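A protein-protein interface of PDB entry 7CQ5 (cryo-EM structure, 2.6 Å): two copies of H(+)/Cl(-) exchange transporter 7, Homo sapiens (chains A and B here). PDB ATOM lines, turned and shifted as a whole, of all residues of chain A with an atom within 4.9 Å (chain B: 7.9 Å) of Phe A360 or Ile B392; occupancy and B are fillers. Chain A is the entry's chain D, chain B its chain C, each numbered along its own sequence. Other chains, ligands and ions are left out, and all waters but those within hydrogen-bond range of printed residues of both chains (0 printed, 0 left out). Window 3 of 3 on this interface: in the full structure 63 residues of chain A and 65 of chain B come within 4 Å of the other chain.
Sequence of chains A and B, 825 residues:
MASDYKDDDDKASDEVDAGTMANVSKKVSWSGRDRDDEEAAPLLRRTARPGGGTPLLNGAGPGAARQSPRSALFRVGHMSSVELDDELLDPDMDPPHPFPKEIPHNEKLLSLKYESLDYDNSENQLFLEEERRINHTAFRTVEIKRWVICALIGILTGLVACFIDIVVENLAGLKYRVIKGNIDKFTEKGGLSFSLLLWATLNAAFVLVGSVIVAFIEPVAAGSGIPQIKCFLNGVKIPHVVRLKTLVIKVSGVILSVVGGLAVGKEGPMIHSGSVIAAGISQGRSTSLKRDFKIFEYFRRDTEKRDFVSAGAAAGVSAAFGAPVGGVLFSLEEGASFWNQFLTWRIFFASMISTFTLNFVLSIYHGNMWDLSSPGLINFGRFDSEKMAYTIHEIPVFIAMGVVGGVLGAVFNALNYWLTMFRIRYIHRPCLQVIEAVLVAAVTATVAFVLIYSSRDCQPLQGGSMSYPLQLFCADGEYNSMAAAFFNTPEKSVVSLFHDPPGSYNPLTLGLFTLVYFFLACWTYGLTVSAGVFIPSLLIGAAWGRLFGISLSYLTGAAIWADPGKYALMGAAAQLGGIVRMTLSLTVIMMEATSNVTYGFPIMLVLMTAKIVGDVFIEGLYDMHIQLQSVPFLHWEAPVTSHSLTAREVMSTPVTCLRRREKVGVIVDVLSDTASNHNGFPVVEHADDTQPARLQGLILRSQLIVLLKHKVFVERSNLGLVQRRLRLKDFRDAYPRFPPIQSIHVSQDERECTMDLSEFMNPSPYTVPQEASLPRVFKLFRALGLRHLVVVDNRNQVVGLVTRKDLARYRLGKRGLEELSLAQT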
ATOM      1  N   PHE A 356      -7.427 -11.197 -20.661  1.00  0.00           N
ATOM      2  CA  PHE A 356      -8.538 -10.842 -19.783  1.00  0.00           C
ATOM      3  C   PHE A 356      -9.880 -10.957 -20.490  1.00  0.00           C
ATOM      4  O   PHE A 356     -10.864 -11.380 -19.879  1.00  0.00           O
ATOM      5  CB  PHE A 356      -8.358  -9.424 -19.242  1.00  0.00           C
ATOM      6  CG  PHE A 356      -9.478  -8.978 -18.346  1.00  0.00           C
ATOM      7  CD1 PHE A 356      -9.576  -9.470 -17.057  1.00  0.00           C
ATOM      8  CD2 PHE A 356     -10.439  -8.083 -18.793  1.00  0.00           C
ATOM      9  CE1 PHE A 356     -10.596  -9.081 -16.229  1.00  0.00           C
ATOM     10  CE2 PHE A 356     -11.471  -7.696 -17.966  1.00  0.00           C
ATOM     11  CZ  PHE A 356     -11.545  -8.195 -16.680  1.00  0.00           C
ATOM     12  N   THR A 357      -9.936 -10.607 -21.777  1.00  0.00           N
ATOM     13  CA  THR A 357     -11.194 -10.658 -22.513  1.00  0.00           C
ATOM     14  C   THR A 357     -11.655 -12.095 -22.724  1.00  0.00           C
ATOM     15  O   THR A 357     -12.840 -12.402 -22.519  1.00  0.00           O
ATOM     16  CB  THR A 357     -11.043  -9.931 -23.850  1.00  0.00           C
ATOM     17  OG1 THR A 357     -10.693  -8.565 -23.608  1.00  0.00           O
ATOM     18  CG2 THR A 357     -12.332  -9.972 -24.636  1.00  0.00           C
ATOM     19  N   LEU A 358     -10.724 -12.986 -23.096  1.00  0.00           N
ATOM     20  CA  LEU A 358     -11.034 -14.412 -23.208  1.00  0.00           C
ATOM     21  C   LEU A 358     -11.541 -14.982 -21.891  1.00  0.00           C
ATOM     22  O   LEU A 358     -12.580 -15.658 -21.853  1.00  0.00           O
ATOM     23  CB  LEU A 358      -9.798 -15.184 -23.651  1.00  0.00           C
ATOM     24  CG  LEU A 358      -9.963 -16.706 -23.656  1.00  0.00           C
ATOM     25  CD1 LEU A 358     -10.844 -17.209 -24.768  1.00  0.00           C
ATOM     26  CD2 LEU A 358      -8.642 -17.371 -23.704  1.00  0.00           C
ATOM     27  N   ASN A 359     -10.832 -14.682 -20.797  1.00  0.00           N
ATOM     28  CA  ASN A 359     -11.182 -15.226 -19.490  1.00  0.00           C
ATOM     29  C   ASN A 359     -12.531 -14.701 -19.010  1.00  0.00           C
ATOM     30  O   ASN A 359     -13.345 -15.460 -18.470  1.00  0.00           O
ATOM     31  CB  ASN A 359     -10.076 -14.872 -18.499  1.00  0.00           C
ATOM     32  CG  ASN A 359     -10.119 -15.701 -17.247  1.00  0.00           C
ATOM     33  OD1 ASN A 359     -10.991 -16.542 -17.069  1.00  0.00           O
ATOM     34  ND2 ASN A 359      -9.145 -15.492 -16.377  1.00  0.00           N
ATOM     35  N   PHE A 360     -12.800 -13.420 -19.255  1.00  0.00           N
ATOM     36  CA  PHE A 360     -14.021 -12.797 -18.769  1.00  0.00           C
ATOM     37  C   PHE A 360     -15.240 -13.259 -19.553  1.00  0.00           C
ATOM     38  O   PHE A 360     -16.318 -13.429 -18.978  1.00  0.00           O
ATOM     39  CB  PHE A 360     -13.875 -11.281 -18.835  1.00  0.00           C
ATOM     40  CG  PHE A 360     -15.088 -10.539 -18.391  1.00  0.00           C
ATOM     41  CD1 PHE A 360     -15.444 -10.514 -17.057  1.00  0.00           C
ATOM     42  CD2 PHE A 360     -15.853  -9.840 -19.303  1.00  0.00           C
ATOM     43  CE1 PHE A 360     -16.558  -9.826 -16.643  1.00  0.00           C
ATOM     44  CE2 PHE A 360     -16.965  -9.146 -18.895  1.00  0.00           C
ATOM     45  CZ  PHE A 360     -17.317  -9.140 -17.563  1.00  0.00           C
ATOM     46  N   VAL A 361     -15.102 -13.470 -20.862  1.00  0.00           N
ATOM     47  CA  VAL A 361     -16.270 -13.929 -21.603  1.00  0.00           C
ATOM     48  C   VAL A 361     -16.489 -15.427 -21.392  1.00  0.00           C
ATOM     49  O   VAL A 361     -17.636 -15.885 -21.350  1.00  0.00           O
ATOM     50  CB  VAL A 361     -16.142 -13.529 -23.086  1.00  0.00           C
ATOM     51  CG1 VAL A 361     -17.302 -14.033 -23.927  1.00  0.00           C
ATOM     52  CG2 VAL A 361     -16.049 -12.026 -23.206  1.00  0.00           C
ATOM     53  N   LEU A 362     -15.430 -16.214 -21.171  1.00  0.00           N
ATOM     54  CA  LEU A 362     -15.668 -17.628 -20.892  1.00  0.00           C
ATOM     55  C   LEU A 362     -16.182 -17.875 -19.481  1.00  0.00           C
ATOM     56  O   LEU A 362     -16.872 -18.871 -19.255  1.00  0.00           O
ATOM     57  CB  LEU A 362     -14.412 -18.463 -21.124  1.00  0.00           C
ATOM     58  CG  LEU A 362     -13.983 -18.680 -22.571  1.00  0.00           C
ATOM     59  CD1 LEU A 362     -12.750 -19.553 -22.602  1.00  0.00           C
ATOM     60  CD2 LEU A 362     -15.103 -19.291 -23.383  1.00  0.00           C
ATOM     61  N   SER A 363     -15.870 -17.004 -18.523  1.00  0.00           N
ATOM     62  CA  SER A 363     -16.436 -17.192 -17.193  1.00  0.00           C
ATOM     63  C   SER A 363     -17.901 -16.780 -17.121  1.00  0.00           C
ATOM     64  O   SER A 363     -18.635 -17.288 -16.269  1.00  0.00           O
ATOM     65  CB  SER A 363     -15.617 -16.426 -16.158  1.00  0.00           C
ATOM     66  OG  SER A 363     -14.323 -16.984 -16.038  1.00  0.00           O
ATOM     67  N   ILE A 364     -18.347 -15.872 -17.990  1.00  0.00           N
ATOM     68  CA  ILE A 364     -19.775 -15.587 -18.089  1.00  0.00           C
ATOM     69  C   ILE A 364     -20.505 -16.776 -18.699  1.00  0.00           C
ATOM     70  O   ILE A 364     -21.582 -17.169 -18.236  1.00  0.00           O
ATOM     71  CB  ILE A 364     -20.008 -14.291 -18.891  1.00  0.00           C
ATOM     72  CG1 ILE A 364     -19.469 -13.079 -18.136  1.00  0.00           C
ATOM     73  CG2 ILE A 364     -21.479 -14.073 -19.191  1.00  0.00           C
ATOM     74  CD1 ILE A 364     -19.445 -11.816 -18.948  1.00  0.00           C
ATOM     75  N   MET A 369     -18.853 -16.042 -13.574  1.00  0.00           N
ATOM     76  CA  MET A 369     -18.397 -14.662 -13.817  1.00  0.00           C
ATOM     77  C   MET A 369     -17.547 -14.113 -12.661  1.00  0.00           C
ATOM     78  O   MET A 369     -16.836 -13.118 -12.824  1.00  0.00           O
ATOM     79  CB  MET A 369     -19.595 -13.740 -14.149  1.00  0.00           C
ATOM     80  CG  MET A 369     -19.308 -12.298 -14.573  1.00  0.00           C
ATOM     81  SD  MET A 369     -20.791 -11.377 -15.021  1.00  0.00           S
ATOM     82  CE  MET A 369     -20.113  -9.743 -15.296  1.00  0.00           C
ATOM     83  N   LEU A 372     -12.427 -16.093 -12.555  1.00  0.00           N
ATOM     84  CA  LEU A 372     -11.591 -15.897 -13.732  1.00  0.00           C
ATOM     85  C   LEU A 372     -10.561 -17.024 -13.744  1.00  0.00           C
ATOM     86  O   LEU A 372      -9.416 -16.877 -13.316  1.00  0.00           O
ATOM     87  CB  LEU A 372     -10.948 -14.520 -13.691  1.00  0.00           C
ATOM     88  CG  LEU A 372     -11.945 -13.366 -13.739  1.00  0.00           C
ATOM     89  CD1 LEU A 372     -11.238 -12.040 -13.537  1.00  0.00           C
ATOM     90  CD2 LEU A 372     -12.698 -13.371 -15.049  1.00  0.00           C
ATOM     91  N   TYR B 390     -10.525 -10.806  -8.466  1.00  0.00           N
ATOM     92  CA  TYR B 390     -11.057  -9.499  -8.810  1.00  0.00           C
ATOM     93  C   TYR B 390     -12.119  -9.634  -9.888  1.00  0.00           C
ATOM     94  O   TYR B 390     -12.249 -10.668 -10.545  1.00  0.00           O
ATOM     95  CB  TYR B 390      -9.946  -8.542  -9.263  1.00  0.00           C
ATOM     96  CG  TYR B 390      -9.284  -8.874 -10.582  1.00  0.00           C
ATOM     97  CD1 TYR B 390      -8.229  -9.771 -10.645  1.00  0.00           C
ATOM     98  CD2 TYR B 390      -9.686  -8.252 -11.757  1.00  0.00           C
ATOM     99  CE1 TYR B 390      -7.617 -10.063 -11.845  1.00  0.00           C
ATOM    100  CE2 TYR B 390      -9.084  -8.538 -12.955  1.00  0.00           C
ATOM    101  CZ  TYR B 390      -8.049  -9.443 -12.996  1.00  0.00           C
ATOM    102  OH  TYR B 390      -7.443  -9.725 -14.195  1.00  0.00           O
ATOM    103  N   THR B 391     -12.890  -8.570 -10.050  1.00  0.00           N
ATOM    104  CA  THR B 391     -13.973  -8.496 -11.017  1.00  0.00           C
ATOM    105  C   THR B 391     -13.705  -7.346 -11.980  1.00  0.00           C
ATOM    106  O   THR B 391     -12.641  -6.724 -11.955  1.00  0.00           O
ATOM    107  CB  THR B 391     -15.314  -8.304 -10.317  1.00  0.00           C
ATOM    108  OG1 THR B 391     -15.281  -7.061  -9.614  1.00  0.00           O
ATOM    109  CG2 THR B 391     -15.567  -9.417  -9.328  1.00  0.00           C
ATOM    110  N   ILE B 392     -14.690  -7.058 -12.827  1.00  0.00           N
ATOM    111  CA  ILE B 392     -14.546  -6.012 -13.828  1.00  0.00           C
ATOM    112  C   ILE B 392     -15.120  -4.675 -13.354  1.00  0.00           C
ATOM    113  O   ILE B 392     -14.755  -3.626 -13.906  1.00  0.00           O
ATOM    114  CB  ILE B 392     -15.186  -6.463 -15.164  1.00  0.00           C
ATOM    115  CG1 ILE B 392     -14.648  -5.660 -16.356  1.00  0.00           C
ATOM    116  CG2 ILE B 392     -16.703  -6.374 -15.111  1.00  0.00           C
ATOM    117  CD1 ILE B 392     -14.979  -6.255 -17.691  1.00  0.00           C
ATOM    118  N   HIS B 393     -15.970  -4.667 -12.323  1.00  0.00           N
ATOM    119  CA  HIS B 393     -16.538  -3.397 -11.887  1.00  0.00           C
ATOM    120  C   HIS B 393     -15.633  -2.655 -10.917  1.00  0.00           C
ATOM    121  O   HIS B 393     -15.822  -1.452 -10.713  1.00  0.00           O
ATOM    122  CB  HIS B 393     -17.919  -3.594 -11.254  1.00  0.00           C
ATOM    123  CG  HIS B 393     -17.895  -4.264  -9.918  1.00  0.00           C
ATOM    124  ND1 HIS B 393     -17.855  -5.633  -9.764  1.00  0.00           N
ATOM    125  CD2 HIS B 393     -17.924  -3.747  -8.667  1.00  0.00           C
ATOM    126  CE1 HIS B 393     -17.863  -5.928  -8.476  1.00  0.00           C
ATOM    127  NE2 HIS B 393     -17.899  -4.802  -7.789  1.00  0.00           N
ATOM    128  N   GLU B 394     -14.658  -3.331 -10.319  1.00  0.00           N
ATOM    129  CA  GLU B 394     -13.657  -2.661  -9.507  1.00  0.00           C
ATOM    130  C   GLU B 394     -12.399  -2.351 -10.297  1.00  0.00           C
ATOM    131  O   GLU B 394     -11.369  -2.026  -9.702  1.00  0.00           O
ATOM    132  CB  GLU B 394     -13.332  -3.489  -8.268  1.00  0.00           C
ATOM    133  CG  GLU B 394     -12.734  -4.833  -8.538  1.00  0.00           C
ATOM    134  CD  GLU B 394     -12.579  -5.623  -7.266  1.00  0.00           C
ATOM    135  OE1 GLU B 394     -12.953  -5.108  -6.198  1.00  0.00           O
ATOM    136  OE2 GLU B 394     -12.087  -6.759  -7.320  1.00  0.00           O
ATOM    137  N   ILE B 395     -12.465  -2.455 -11.623  1.00  0.00           N
ATOM    138  CA  ILE B 395     -11.421  -1.870 -12.467  1.00  0.00           C
ATOM    139  C   ILE B 395     -11.300  -0.358 -12.299  1.00  0.00           C
ATOM    140  O   ILE B 395     -10.167   0.121 -12.146  1.00  0.00           O
ATOM    141  CB  ILE B 395     -11.605  -2.322 -13.923  1.00  0.00           C
ATOM    142  CG1 ILE B 395     -11.454  -3.841 -14.026  1.00  0.00           C
ATOM    143  CG2 ILE B 395     -10.649  -1.613 -14.864  1.00  0.00           C
ATOM    144  CD1 ILE B 395     -10.123  -4.354 -13.547  1.00  0.00           C
ATOM    145  N   PRO B 396     -12.377   0.457 -12.275  1.00  0.00           N
ATOM    146  CA  PRO B 396     -12.157   1.886 -11.979  1.00  0.00           C
ATOM    147  C   PRO B 396     -11.841   2.189 -10.521  1.00  0.00           C
ATOM    148  O   PRO B 396     -11.379   3.298 -10.233  1.00  0.00           O
ATOM    149  CB  PRO B 396     -13.471   2.548 -12.407  1.00  0.00           C
ATOM    150  CG  PRO B 396     -14.459   1.514 -12.278  1.00  0.00           C
ATOM    151  CD  PRO B 396     -13.784   0.257 -12.694  1.00  0.00           C
ATOM    152  N   VAL B 397     -12.080   1.262  -9.592  1.00  0.00           N
ATOM    153  CA  VAL B 397     -11.588   1.454  -8.230  1.00  0.00           C
ATOM    154  C   VAL B 397     -10.073   1.309  -8.214  1.00  0.00           C
ATOM    155  O   VAL B 397      -9.375   1.998  -7.459  1.00  0.00           O
ATOM    156  CB  VAL B 397     -12.283   0.463  -7.273  1.00  0.00           C
ATOM    157  CG1 VAL B 397     -11.780   0.601  -5.843  1.00  0.00           C
ATOM    158  CG2 VAL B 397     -13.783   0.645  -7.320  1.00  0.00           C
ATOM    159  N   PHE B 398      -9.539   0.454  -9.084  1.00  0.00           N
ATOM    160  CA  PHE B 398      -8.098   0.295  -9.203  1.00  0.00           C
ATOM    161  C   PHE B 398      -7.447   1.495  -9.886  1.00  0.00           C
ATOM    162  O   PHE B 398      -6.324   1.862  -9.532  1.00  0.00           O
ATOM    163  CB  PHE B 398      -7.792  -0.993  -9.965  1.00  0.00           C
ATOM    164  CG  PHE B 398      -8.149  -2.246  -9.216  1.00  0.00           C
ATOM    165  CD1 PHE B 398      -8.218  -2.254  -7.834  1.00  0.00           C
ATOM    166  CD2 PHE B 398      -8.468  -3.406  -9.901  1.00  0.00           C
ATOM    167  CE1 PHE B 398      -8.554  -3.401  -7.152  1.00  0.00           C
ATOM    168  CE2 PHE B 398      -8.817  -4.559  -9.223  1.00  0.00           C
ATOM    169  CZ  PHE B 398      -8.861  -4.555  -7.849  1.00  0.00           C
ATOM    170  N   PHE B 601      -3.358  -7.547 -15.391  1.00  0.00           N
ATOM    171  CA  PHE B 601      -4.214  -6.544 -15.998  1.00  0.00           C
ATOM    172  C   PHE B 601      -4.479  -5.374 -15.039  1.00  0.00           C
ATOM    173  O   PHE B 601      -4.213  -4.227 -15.439  1.00  0.00           O
ATOM    174  CB  PHE B 601      -5.484  -7.211 -16.549  1.00  0.00           C
ATOM    175  CG  PHE B 601      -6.455  -6.257 -17.138  1.00  0.00           C
ATOM    176  CD1 PHE B 601      -6.110  -5.508 -18.237  1.00  0.00           C
ATOM    177  CD2 PHE B 601      -7.733  -6.149 -16.631  1.00  0.00           C
ATOM    178  CE1 PHE B 601      -6.995  -4.630 -18.782  1.00  0.00           C
ATOM    179  CE2 PHE B 601      -8.634  -5.278 -17.190  1.00  0.00           C
ATOM    180  CZ  PHE B 601      -8.259  -4.519 -18.273  1.00  0.00           C
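No position is printed for both chains.
The side-chain amide nitrogen of Asn A359 lies close to the backbone carbonyl oxygen of Leu A372, 3.4 Å away.
Of the printed residues of chain B, Phe A356 touches Tyr B390, Ile B392 and Phe B601.
Of chain B, only Ile B392 comes within 4 Å of Phe A360.
Met A369 touches none of the printed residues of chain B.
Ile B392 touches two residues of chain A.
Of the printed residues of chain A, Phe B601 touches Phe A356 (3.7 Å).
The nearest residue of chain B that does not touch Phe A360 is Thr B391 (6.0 Å).
The nearest residue of chain A that does not touch Ile B392 is Met A369 (4.8 Å).
The nearest printed residue of chain A that does not touch Phe B601 is Thr A357 (7.1 Å).
Phe A356 touches Tyr B390 (CD1 to OH, 3.6 Å).
CD1 of Ile B392 touches CE2 of Phe A356, at 3.8 Å.
Phe A356 touches Phe B601.
CE2 of Phe A360 touches CD1 of Ile B392, 3.7 Å away.
CD1 of Leu A372 touches O of Tyr B390, at 3.4 Å.
Hydrophobic or aromatic side chains of chain A that line the printed part of chain B: Phe A356, Phe A360 and Leu A372.
Among the printed residues, no Asp or Glu carboxylate lies within 4 Å of a Lys or Arg side-chain nitrogen of the other chain.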
